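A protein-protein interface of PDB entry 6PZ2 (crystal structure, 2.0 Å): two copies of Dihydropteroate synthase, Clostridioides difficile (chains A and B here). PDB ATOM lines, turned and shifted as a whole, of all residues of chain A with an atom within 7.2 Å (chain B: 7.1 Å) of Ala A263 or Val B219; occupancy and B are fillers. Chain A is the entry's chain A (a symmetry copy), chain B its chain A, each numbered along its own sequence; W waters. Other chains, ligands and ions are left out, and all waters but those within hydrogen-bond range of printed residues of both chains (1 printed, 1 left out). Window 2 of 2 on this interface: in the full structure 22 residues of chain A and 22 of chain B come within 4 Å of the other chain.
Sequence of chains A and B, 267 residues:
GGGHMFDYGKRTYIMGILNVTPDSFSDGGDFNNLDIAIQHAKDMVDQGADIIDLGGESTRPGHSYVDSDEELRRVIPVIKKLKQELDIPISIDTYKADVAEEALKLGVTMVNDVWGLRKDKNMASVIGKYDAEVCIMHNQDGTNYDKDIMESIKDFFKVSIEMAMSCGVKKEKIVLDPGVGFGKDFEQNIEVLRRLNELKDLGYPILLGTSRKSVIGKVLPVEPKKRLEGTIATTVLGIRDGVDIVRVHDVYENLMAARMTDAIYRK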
ATOM      1  N   MET A 256       4.959   1.320 -12.826  1.00  0.00           N
ATOM      2  CA  MET A 256       5.579   0.587 -11.703  1.00  0.00           C
ATOM      3  C   MET A 256       6.973   0.101 -12.122  1.00  0.00           C
ATOM      4  O   MET A 256       7.932   0.324 -11.403  1.00  0.00           O
ATOM      5  CB  MET A 256       4.731  -0.605 -11.237  1.00  0.00           C
ATOM      6  CG  MET A 256       3.390  -0.238 -10.653  1.00  0.00           C
ATOM      7  SD  MET A 256       3.573   0.972  -9.321  1.00  0.00           S
ATOM      8  CE  MET A 256       3.062   2.518 -10.060  1.00  0.00           C
ATOM      9  N   ALA A 257       7.124  -0.476 -13.326  1.00  0.00           N
ATOM     10  CA  ALA A 257       8.427  -0.910 -13.828  1.00  0.00           C
ATOM     11  C   ALA A 257       9.392   0.274 -14.003  1.00  0.00           C
ATOM     12  O   ALA A 257      10.623   0.176 -13.759  1.00  0.00           O
ATOM     13  CB  ALA A 257       8.216  -1.656 -15.146  1.00  0.00           C
ATOM     14  N   ALA A 258       8.854   1.398 -14.479  1.00  0.00           N
ATOM     15  CA  ALA A 258       9.657   2.580 -14.696  1.00  0.00           C
ATOM     16  C   ALA A 258      10.186   3.106 -13.355  1.00  0.00           C
ATOM     17  O   ALA A 258      11.300   3.571 -13.287  1.00  0.00           O
ATOM     18  CB  ALA A 258       8.829   3.650 -15.379  1.00  0.00           C
ATOM     19  N   ARG A 259       9.381   3.065 -12.313  1.00  0.00           N
ATOM     20  CA  ARG A 259       9.867   3.550 -10.994  1.00  0.00           C
ATOM     21  C   ARG A 259      10.999   2.658 -10.477  1.00  0.00           C
ATOM     22  O   ARG A 259      11.965   3.160  -9.947  1.00  0.00           O
ATOM     23  CB  ARG A 259       8.712   3.557  -9.996  1.00  0.00           C
ATOM     24  CG  ARG A 259       7.735   4.684 -10.281  1.00  0.00           C
ATOM     25  CD  ARG A 259       6.679   4.792  -9.210  1.00  0.00           C
ATOM     26  NE  ARG A 259       5.826   5.937  -9.434  1.00  0.00           N
ATOM     27  CZ  ARG A 259       4.693   6.165  -8.775  1.00  0.00           C
ATOM     28  NH1 ARG A 259       4.005   7.267  -9.019  1.00  0.00           N
ATOM     29  NH2 ARG A 259       4.269   5.312  -7.855  1.00  0.00           N
ATOM     30  N   MET A 260      10.921   1.351 -10.750  1.00  0.00           N
ATOM     31  CA  MET A 260      11.928   0.437 -10.282  1.00  0.00           C
ATOM     32  C   MET A 260      13.208   0.739 -11.053  1.00  0.00           C
ATOM     33  O   MET A 260      14.267   0.875 -10.468  1.00  0.00           O
ATOM     34  CB  MET A 260      11.495  -1.029 -10.441  1.00  0.00           C
ATOM     35  CG  MET A 260      12.422  -2.013  -9.729  1.00  0.00           C
ATOM     36  SD  MET A 260      12.448  -1.718  -7.918  1.00  0.00           S
ATOM     37  CE  MET A 260      14.175  -2.000  -7.550  1.00  0.00           C
ATOM     38  N   THR A 261      13.080   0.944 -12.360  1.00  0.00           N
ATOM     39  CA  THR A 261      14.241   1.250 -13.161  1.00  0.00           C
ATOM     40  C   THR A 261      14.811   2.625 -12.788  1.00  0.00           C
ATOM     41  O   THR A 261      16.037   2.807 -12.718  1.00  0.00           O
ATOM     42  CB  THR A 261      13.881   1.169 -14.652  1.00  0.00           C
ATOM     43  OG1 THR A 261      13.117  -0.011 -14.922  1.00  0.00           O
ATOM     44  CG2 THR A 261      15.119   1.215 -15.503  1.00  0.00           C
ATOM     45  N   ASP A 262      13.934   3.598 -12.563  1.00  0.00           N
ATOM     46  CA  ASP A 262      14.404   4.947 -12.184  1.00  0.00           C
ATOM     47  C   ASP A 262      15.236   4.830 -10.900  1.00  0.00           C
ATOM     48  O   ASP A 262      16.275   5.469 -10.787  1.00  0.00           O
ATOM     49  CB  ASP A 262      13.266   5.955 -11.930  1.00  0.00           C
ATOM     50  CG  ASP A 262      12.484   6.383 -13.165  1.00  0.00           C
ATOM     51  OD1 ASP A 262      13.019   6.196 -14.299  1.00  0.00           O
ATOM     52  OD2 ASP A 262      11.328   6.851 -12.986  1.00  0.00           O
ATOM     53  N   ALA A 263      14.783   4.021  -9.937  1.00  0.00           N
ATOM     54  CA  ALA A 263      15.493   3.929  -8.631  1.00  0.00           C
ATOM     55  C   ALA A 263      16.894   3.338  -8.822  1.00  0.00           C
ATOM     56  O   ALA A 263      17.815   3.707  -8.125  1.00  0.00           O
ATOM     57  CB  ALA A 263      14.678   3.114  -7.664  1.00  0.00           C
ATOM     58  N   ILE A 264      17.094   2.500  -9.834  1.00  0.00           N
ATOM     59  CA  ILE A 264      18.410   1.905 -10.068  1.00  0.00           C
ATOM     60  C   ILE A 264      19.333   2.855 -10.855  1.00  0.00           C
ATOM     61  O   ILE A 264      20.518   2.905 -10.572  1.00  0.00           O
ATOM     62  CB  ILE A 264      18.240   0.548 -10.786  1.00  0.00           C
ATOM     63  CG1 ILE A 264      17.459  -0.455  -9.933  1.00  0.00           C
ATOM     64  CG2 ILE A 264      19.575  -0.027 -11.239  1.00  0.00           C
ATOM     65  CD1 ILE A 264      16.963  -1.660 -10.715  1.00  0.00           C
ATOM     66  N   TYR A 265      18.866   3.582 -11.869  1.00  0.00           N
ATOM     67  CA  TYR A 265      19.784   4.338 -12.731  1.00  0.00           C
ATOM     68  C   TYR A 265      19.708   5.859 -12.574  1.00  0.00           C
ATOM     69  O   TYR A 265      20.566   6.538 -13.086  1.00  0.00           O
ATOM     70  CB  TYR A 265      19.497   4.051 -14.202  1.00  0.00           C
ATOM     71  CG  TYR A 265      19.804   2.615 -14.508  1.00  0.00           C
ATOM     72  CD1 TYR A 265      21.115   2.186 -14.619  1.00  0.00           C
ATOM     73  CD2 TYR A 265      18.800   1.674 -14.506  1.00  0.00           C
ATOM     74  CE1 TYR A 265      21.421   0.848 -14.814  1.00  0.00           C
ATOM     75  CE2 TYR A 265      19.090   0.333 -14.680  1.00  0.00           C
ATOM     76  CZ  TYR A 265      20.401  -0.082 -14.837  1.00  0.00           C
ATOM     77  OH  TYR A 265      20.672  -1.394 -15.066  1.00  0.00           O
ATOM     78  N   ARG A 266      18.658   6.423 -12.024  1.00  0.00           N
ATOM     79  CA  ARG A 266      18.553   7.884 -12.016  1.00  0.00           C
ATOM     80  C   ARG A 266      19.056   8.342 -10.647  1.00  0.00           C
ATOM     81  O   ARG A 266      18.834   7.636  -9.667  1.00  0.00           O
ATOM     82  CB  ARG A 266      17.121   8.349 -12.303  1.00  0.00           C
ATOM     83  CG  ARG A 266      16.716   8.201 -13.764  1.00  0.00           C
ATOM     84  CD  ARG A 266      15.361   8.810 -14.057  1.00  0.00           C
ATOM     85  NE  ARG A 266      14.732   8.250 -15.250  1.00  0.00           N
ATOM     86  CZ  ARG A 266      14.930   8.718 -16.473  1.00  0.00           C
ATOM     87  NH1 ARG A 266      14.145   8.350 -17.485  1.00  0.00           N
ATOM     88  NH2 ARG A 266      15.930   9.566 -16.640  1.00  0.00           N
ATOM     89  N   LYS A 267      19.696   9.502 -10.602  1.00  0.00           N
ATOM     90  CA  LYS A 267      20.597   9.838  -9.499  1.00  0.00           C
ATOM     91  C   LYS A 267      19.767  10.477  -8.374  1.00  0.00           C
ATOM     92  O   LYS A 267      18.859   9.850  -7.800  1.00  0.00           O
ATOM     93  CB  LYS A 267      21.744  10.735  -9.995  1.00  0.00           C
ATOM     94  CG  LYS A 267      22.086  10.681 -11.485  1.00  0.00           C
ATOM     95  CD  LYS A 267      23.338   9.895 -11.841  1.00  0.00           C
ATOM     96  CE  LYS A 267      23.124   8.398 -11.898  1.00  0.00           C
ATOM     97  NZ  LYS A 267      23.231   7.773 -10.556  1.00  0.00           N
ATOM     98  OXT LYS A 267      19.969  11.639  -8.006  1.00  0.00           O
ATOM     99  N   PHE B 186      18.970  -1.157   1.489  1.00  0.00           N
ATOM    100  CA  PHE B 186      18.302  -0.693   0.278  1.00  0.00           C
ATOM    101  C   PHE B 186      19.323  -0.163  -0.731  1.00  0.00           C
ATOM    102  O   PHE B 186      19.413  -0.635  -1.870  1.00  0.00           O
ATOM    103  CB  PHE B 186      17.243   0.365   0.595  1.00  0.00           C
ATOM    104  CG  PHE B 186      16.630   0.943  -0.656  1.00  0.00           C
ATOM    105  CD1 PHE B 186      15.788   0.169  -1.445  1.00  0.00           C
ATOM    106  CD2 PHE B 186      16.992   2.207  -1.095  1.00  0.00           C
ATOM    107  CE1 PHE B 186      15.270   0.669  -2.625  1.00  0.00           C
ATOM    108  CE2 PHE B 186      16.447   2.713  -2.263  1.00  0.00           C
ATOM    109  CZ  PHE B 186      15.605   1.944  -3.028  1.00  0.00           C
ATOM    110  N   ILE B 190      20.446  -1.705  -4.349  1.00  0.00           N
ATOM    111  CA  ILE B 190      20.350  -0.858  -5.570  1.00  0.00           C
ATOM    112  C   ILE B 190      21.703  -0.796  -6.285  1.00  0.00           C
ATOM    113  O   ILE B 190      21.857  -0.999  -7.523  1.00  0.00           O
ATOM    114  CB  ILE B 190      19.795   0.534  -5.213  1.00  0.00           C
ATOM    115  CG1 ILE B 190      18.319   0.453  -4.833  1.00  0.00           C
ATOM    116  CG2 ILE B 190      20.034   1.561  -6.315  1.00  0.00           C
ATOM    117  CD1 ILE B 190      17.425  -0.106  -5.900  1.00  0.00           C
ATOM    118  N   GLU B 191      22.724  -0.579  -5.484  1.00  0.00           N
ATOM    119  CA  GLU B 191      24.041  -0.427  -6.049  1.00  0.00           C
ATOM    120  C   GLU B 191      24.510  -1.715  -6.726  1.00  0.00           C
ATOM    121  O   GLU B 191      25.123  -1.694  -7.811  1.00  0.00           O
ATOM    122  CB  GLU B 191      25.033  -0.040  -4.954  1.00  0.00           C
ATOM    123  CG  GLU B 191      26.439  -0.002  -5.522  1.00  0.00           C
ATOM    124  CD  GLU B 191      27.486   0.759  -4.740  1.00  0.00           C
ATOM    125  OE1 GLU B 191      27.201   1.132  -3.577  1.00  0.00           O
ATOM    126  OE2 GLU B 191      28.602   0.900  -5.291  1.00  0.00           O
ATOM    127  N   ARG B 194      22.699  -2.147  -9.961  1.00  0.00           N
ATOM    128  CA  ARG B 194      23.257  -1.183 -10.922  1.00  0.00           C
ATOM    129  C   ARG B 194      24.589  -1.716 -11.472  1.00  0.00           C
ATOM    130  O   ARG B 194      24.868  -1.577 -12.650  1.00  0.00           O
ATOM    131  CB  ARG B 194      23.401   0.185 -10.237  1.00  0.00           C
ATOM    132  CG  ARG B 194      23.560   1.394 -11.153  1.00  0.00           C
ATOM    133  CD  ARG B 194      24.052   2.626 -10.400  1.00  0.00           C
ATOM    134  NE  ARG B 194      23.299   2.949  -9.191  1.00  0.00           N
ATOM    135  CZ  ARG B 194      23.822   3.088  -7.976  1.00  0.00           C
ATOM    136  NH1 ARG B 194      23.033   3.378  -6.951  1.00  0.00           N
ATOM    137  NH2 ARG B 194      25.127   2.962  -7.798  1.00  0.00           N
ATOM    138  N   SER B 214      11.991  -6.860  -0.354  1.00  0.00           N
ATOM    139  CA  SER B 214      11.758  -5.565   0.266  1.00  0.00           C
ATOM    140  C   SER B 214      12.510  -4.466  -0.487  1.00  0.00           C
ATOM    141  O   SER B 214      12.150  -3.309  -0.400  1.00  0.00           O
ATOM    142  CB  SER B 214      12.194  -5.589   1.708  1.00  0.00           C
ATOM    143  OG  SER B 214      13.612  -5.637   1.746  1.00  0.00           O
ATOM    144  N   VAL B 215      13.569  -4.792  -1.208  1.00  0.00           N
ATOM    145  CA  VAL B 215      14.228  -3.770  -2.033  1.00  0.00           C
ATOM    146  C   VAL B 215      13.269  -3.231  -3.110  1.00  0.00           C
ATOM    147  O   VAL B 215      13.318  -2.049  -3.462  1.00  0.00           O
ATOM    148  CB  VAL B 215      15.517  -4.275  -2.706  1.00  0.00           C
ATOM    149  CG1 VAL B 215      15.279  -5.442  -3.660  1.00  0.00           C
ATOM    150  CG2 VAL B 215      16.214  -3.139  -3.447  1.00  0.00           C
ATOM    151  N   ILE B 216      12.407  -4.085  -3.643  1.00  0.00           N
ATOM    152  CA  ILE B 216      11.405  -3.655  -4.580  1.00  0.00           C
ATOM    153  C   ILE B 216      10.276  -2.946  -3.826  1.00  0.00           C
ATOM    154  O   ILE B 216       9.809  -1.886  -4.235  1.00  0.00           O
ATOM    155  CB  ILE B 216      10.892  -4.853  -5.384  1.00  0.00           C
ATOM    156  CG1 ILE B 216      12.043  -5.494  -6.153  1.00  0.00           C
ATOM    157  CG2 ILE B 216       9.762  -4.391  -6.266  1.00  0.00           C
ATOM    158  CD1 ILE B 216      11.631  -6.731  -6.900  1.00  0.00           C
ATOM    159  N   GLY B 217       9.893  -3.490  -2.687  1.00  0.00           N
ATOM    160  CA  GLY B 217       8.805  -2.915  -1.873  1.00  0.00           C
ATOM    161  C   GLY B 217       9.079  -1.500  -1.409  1.00  0.00           C
ATOM    162  O   GLY B 217       8.163  -0.721  -1.130  1.00  0.00           O
ATOM    163  N   LYS B 218      10.340  -1.155  -1.285  1.00  0.00           N
ATOM    164  CA  LYS B 218      10.652   0.179  -0.849  1.00  0.00           C
ATOM    165  C   LYS B 218      10.388   1.159  -2.000  1.00  0.00           C
ATOM    166  O   LYS B 218      10.104   2.302  -1.726  1.00  0.00           O
ATOM    167  CB  LYS B 218      12.107   0.280  -0.394  1.00  0.00           C
ATOM    168  CG  LYS B 218      12.381   1.377   0.624  1.00  0.00           C
ATOM    169  CD  LYS B 218      13.475   1.017   1.617  1.00  0.00           C
ATOM    170  CE  LYS B 218      13.325  -0.347   2.270  1.00  0.00           C
ATOM    171  NZ  LYS B 218      14.222  -0.489   3.445  1.00  0.00           N
ATOM    172  N   VAL B 219      10.475   0.731  -3.262  1.00  0.00           N
ATOM    173  CA  VAL B 219      10.195   1.610  -4.409  1.00  0.00           C
ATOM    174  C   VAL B 219       8.698   1.523  -4.728  1.00  0.00           C
ATOM    175  O   VAL B 219       8.061   2.494  -5.087  1.00  0.00           O
ATOM    176  CB  VAL B 219      11.069   1.223  -5.622  1.00  0.00           C
ATOM    177  CG1 VAL B 219      10.743   2.018  -6.884  1.00  0.00           C
ATOM    178  CG2 VAL B 219      12.540   1.367  -5.293  1.00  0.00           C
ATOM    179  N   LEU B 220       8.135   0.339  -4.569  1.00  0.00           N
ATOM    180  CA  LEU B 220       6.762   0.063  -4.878  1.00  0.00           C
ATOM    181  C   LEU B 220       6.050  -0.448  -3.620  1.00  0.00           C
ATOM    182  O   LEU B 220       5.910  -1.667  -3.468  1.00  0.00           O
ATOM    183  CB  LEU B 220       6.725  -1.009  -5.975  1.00  0.00           C
ATOM    184  CG  LEU B 220       7.552  -0.720  -7.221  1.00  0.00           C
ATOM    185  CD1 LEU B 220       7.420  -1.858  -8.224  1.00  0.00           C
ATOM    186  CD2 LEU B 220       7.099   0.578  -7.864  1.00  0.00           C
ATOM    187  N   PRO B 221       5.573   0.462  -2.734  1.00  0.00           N
ATOM    188  CA  PRO B 221       5.077   0.034  -1.414  1.00  0.00           C
ATOM    189  C   PRO B 221       3.693  -0.616  -1.512  1.00  0.00           C
ATOM    190  O   PRO B 221       2.710  -0.073  -1.048  1.00  0.00           O
ATOM    191  CB  PRO B 221       5.012   1.267  -0.507  1.00  0.00           C
ATOM    192  CG  PRO B 221       5.366   2.439  -1.392  1.00  0.00           C
ATOM    193  CD  PRO B 221       5.801   1.906  -2.745  1.00  0.00           C
ATOM    194  N   VAL B 222       3.639  -1.770  -2.153  1.00  0.00           N
ATOM    195  CA  VAL B 222       2.443  -2.578  -2.186  1.00  0.00           C
ATOM    196  C   VAL B 222       2.831  -3.941  -1.602  1.00  0.00           C
ATOM    197  O   VAL B 222       4.016  -4.223  -1.385  1.00  0.00           O
ATOM    198  CB  VAL B 222       1.885  -2.690  -3.619  1.00  0.00           C
ATOM    199  CG1 VAL B 222       1.531  -1.311  -4.176  1.00  0.00           C
ATOM    200  CG2 VAL B 222       2.857  -3.421  -4.541  1.00  0.00           C
HETATM  201  O   HOH W   1       5.645   3.450  -6.068  1.00  0.00           O
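NE of Arg B194 lies within hydrogen-bond range of O of Ile A264.
O of Met A256 touches CD2 of Leu B220, 3.6 Å away. Arg A259 touches Val B219. SD of Met A260 touches CA of Ile B216, at 3.998 Å. Val B219 touches Met A260 (CG1 to N, 3.9 Å). Ala A263 touches Ile B190 (O to CG2, 3.6 Å). Ala A263 touches Val B219 (CB to CG2, 3.6 Å).
Of the printed residues of chain B, Arg A259 touches Val B219 (3.5 Å). Of the printed residues of chain B, Met A260 touches Ile B216 and Val B219. Ala A263 touches two residues of chain B. Of chain A, only Arg A259, Met A260 and Ala A263 come within 4 Å of Val B219. Val B222 touches none of the printed residues of chain A. The nearest residue of chain B that does not touch Ala A263 is Phe B186 (4.9 Å). The nearest printed residue of chain A that does not touch Arg B194 is Tyr A265 (4.3 Å).
Hydrophobic or aromatic side chains of chain B that line the printed part of chain A: Ile B190, Val B219 and Leu B220. Printed residues of chain A that touch a printed residue of chain B: Met A256, Arg A259, Met A260, Ala A263 and Ile A264. Hydrophobic or aromatic side chains of chain A that line the printed part of chain B: Met A256, Met A260, Ala A263 and Ile A264. Among the printed residues, no Asp or Glu carboxylate lies within 4 Å of a Lys or Arg side-chain nitrogen of the other chain.
No position is printed for both chains.
Water W1 bridges the backbone carbonyl oxygen of Val B219 and the guanidinium group of Arg A259.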
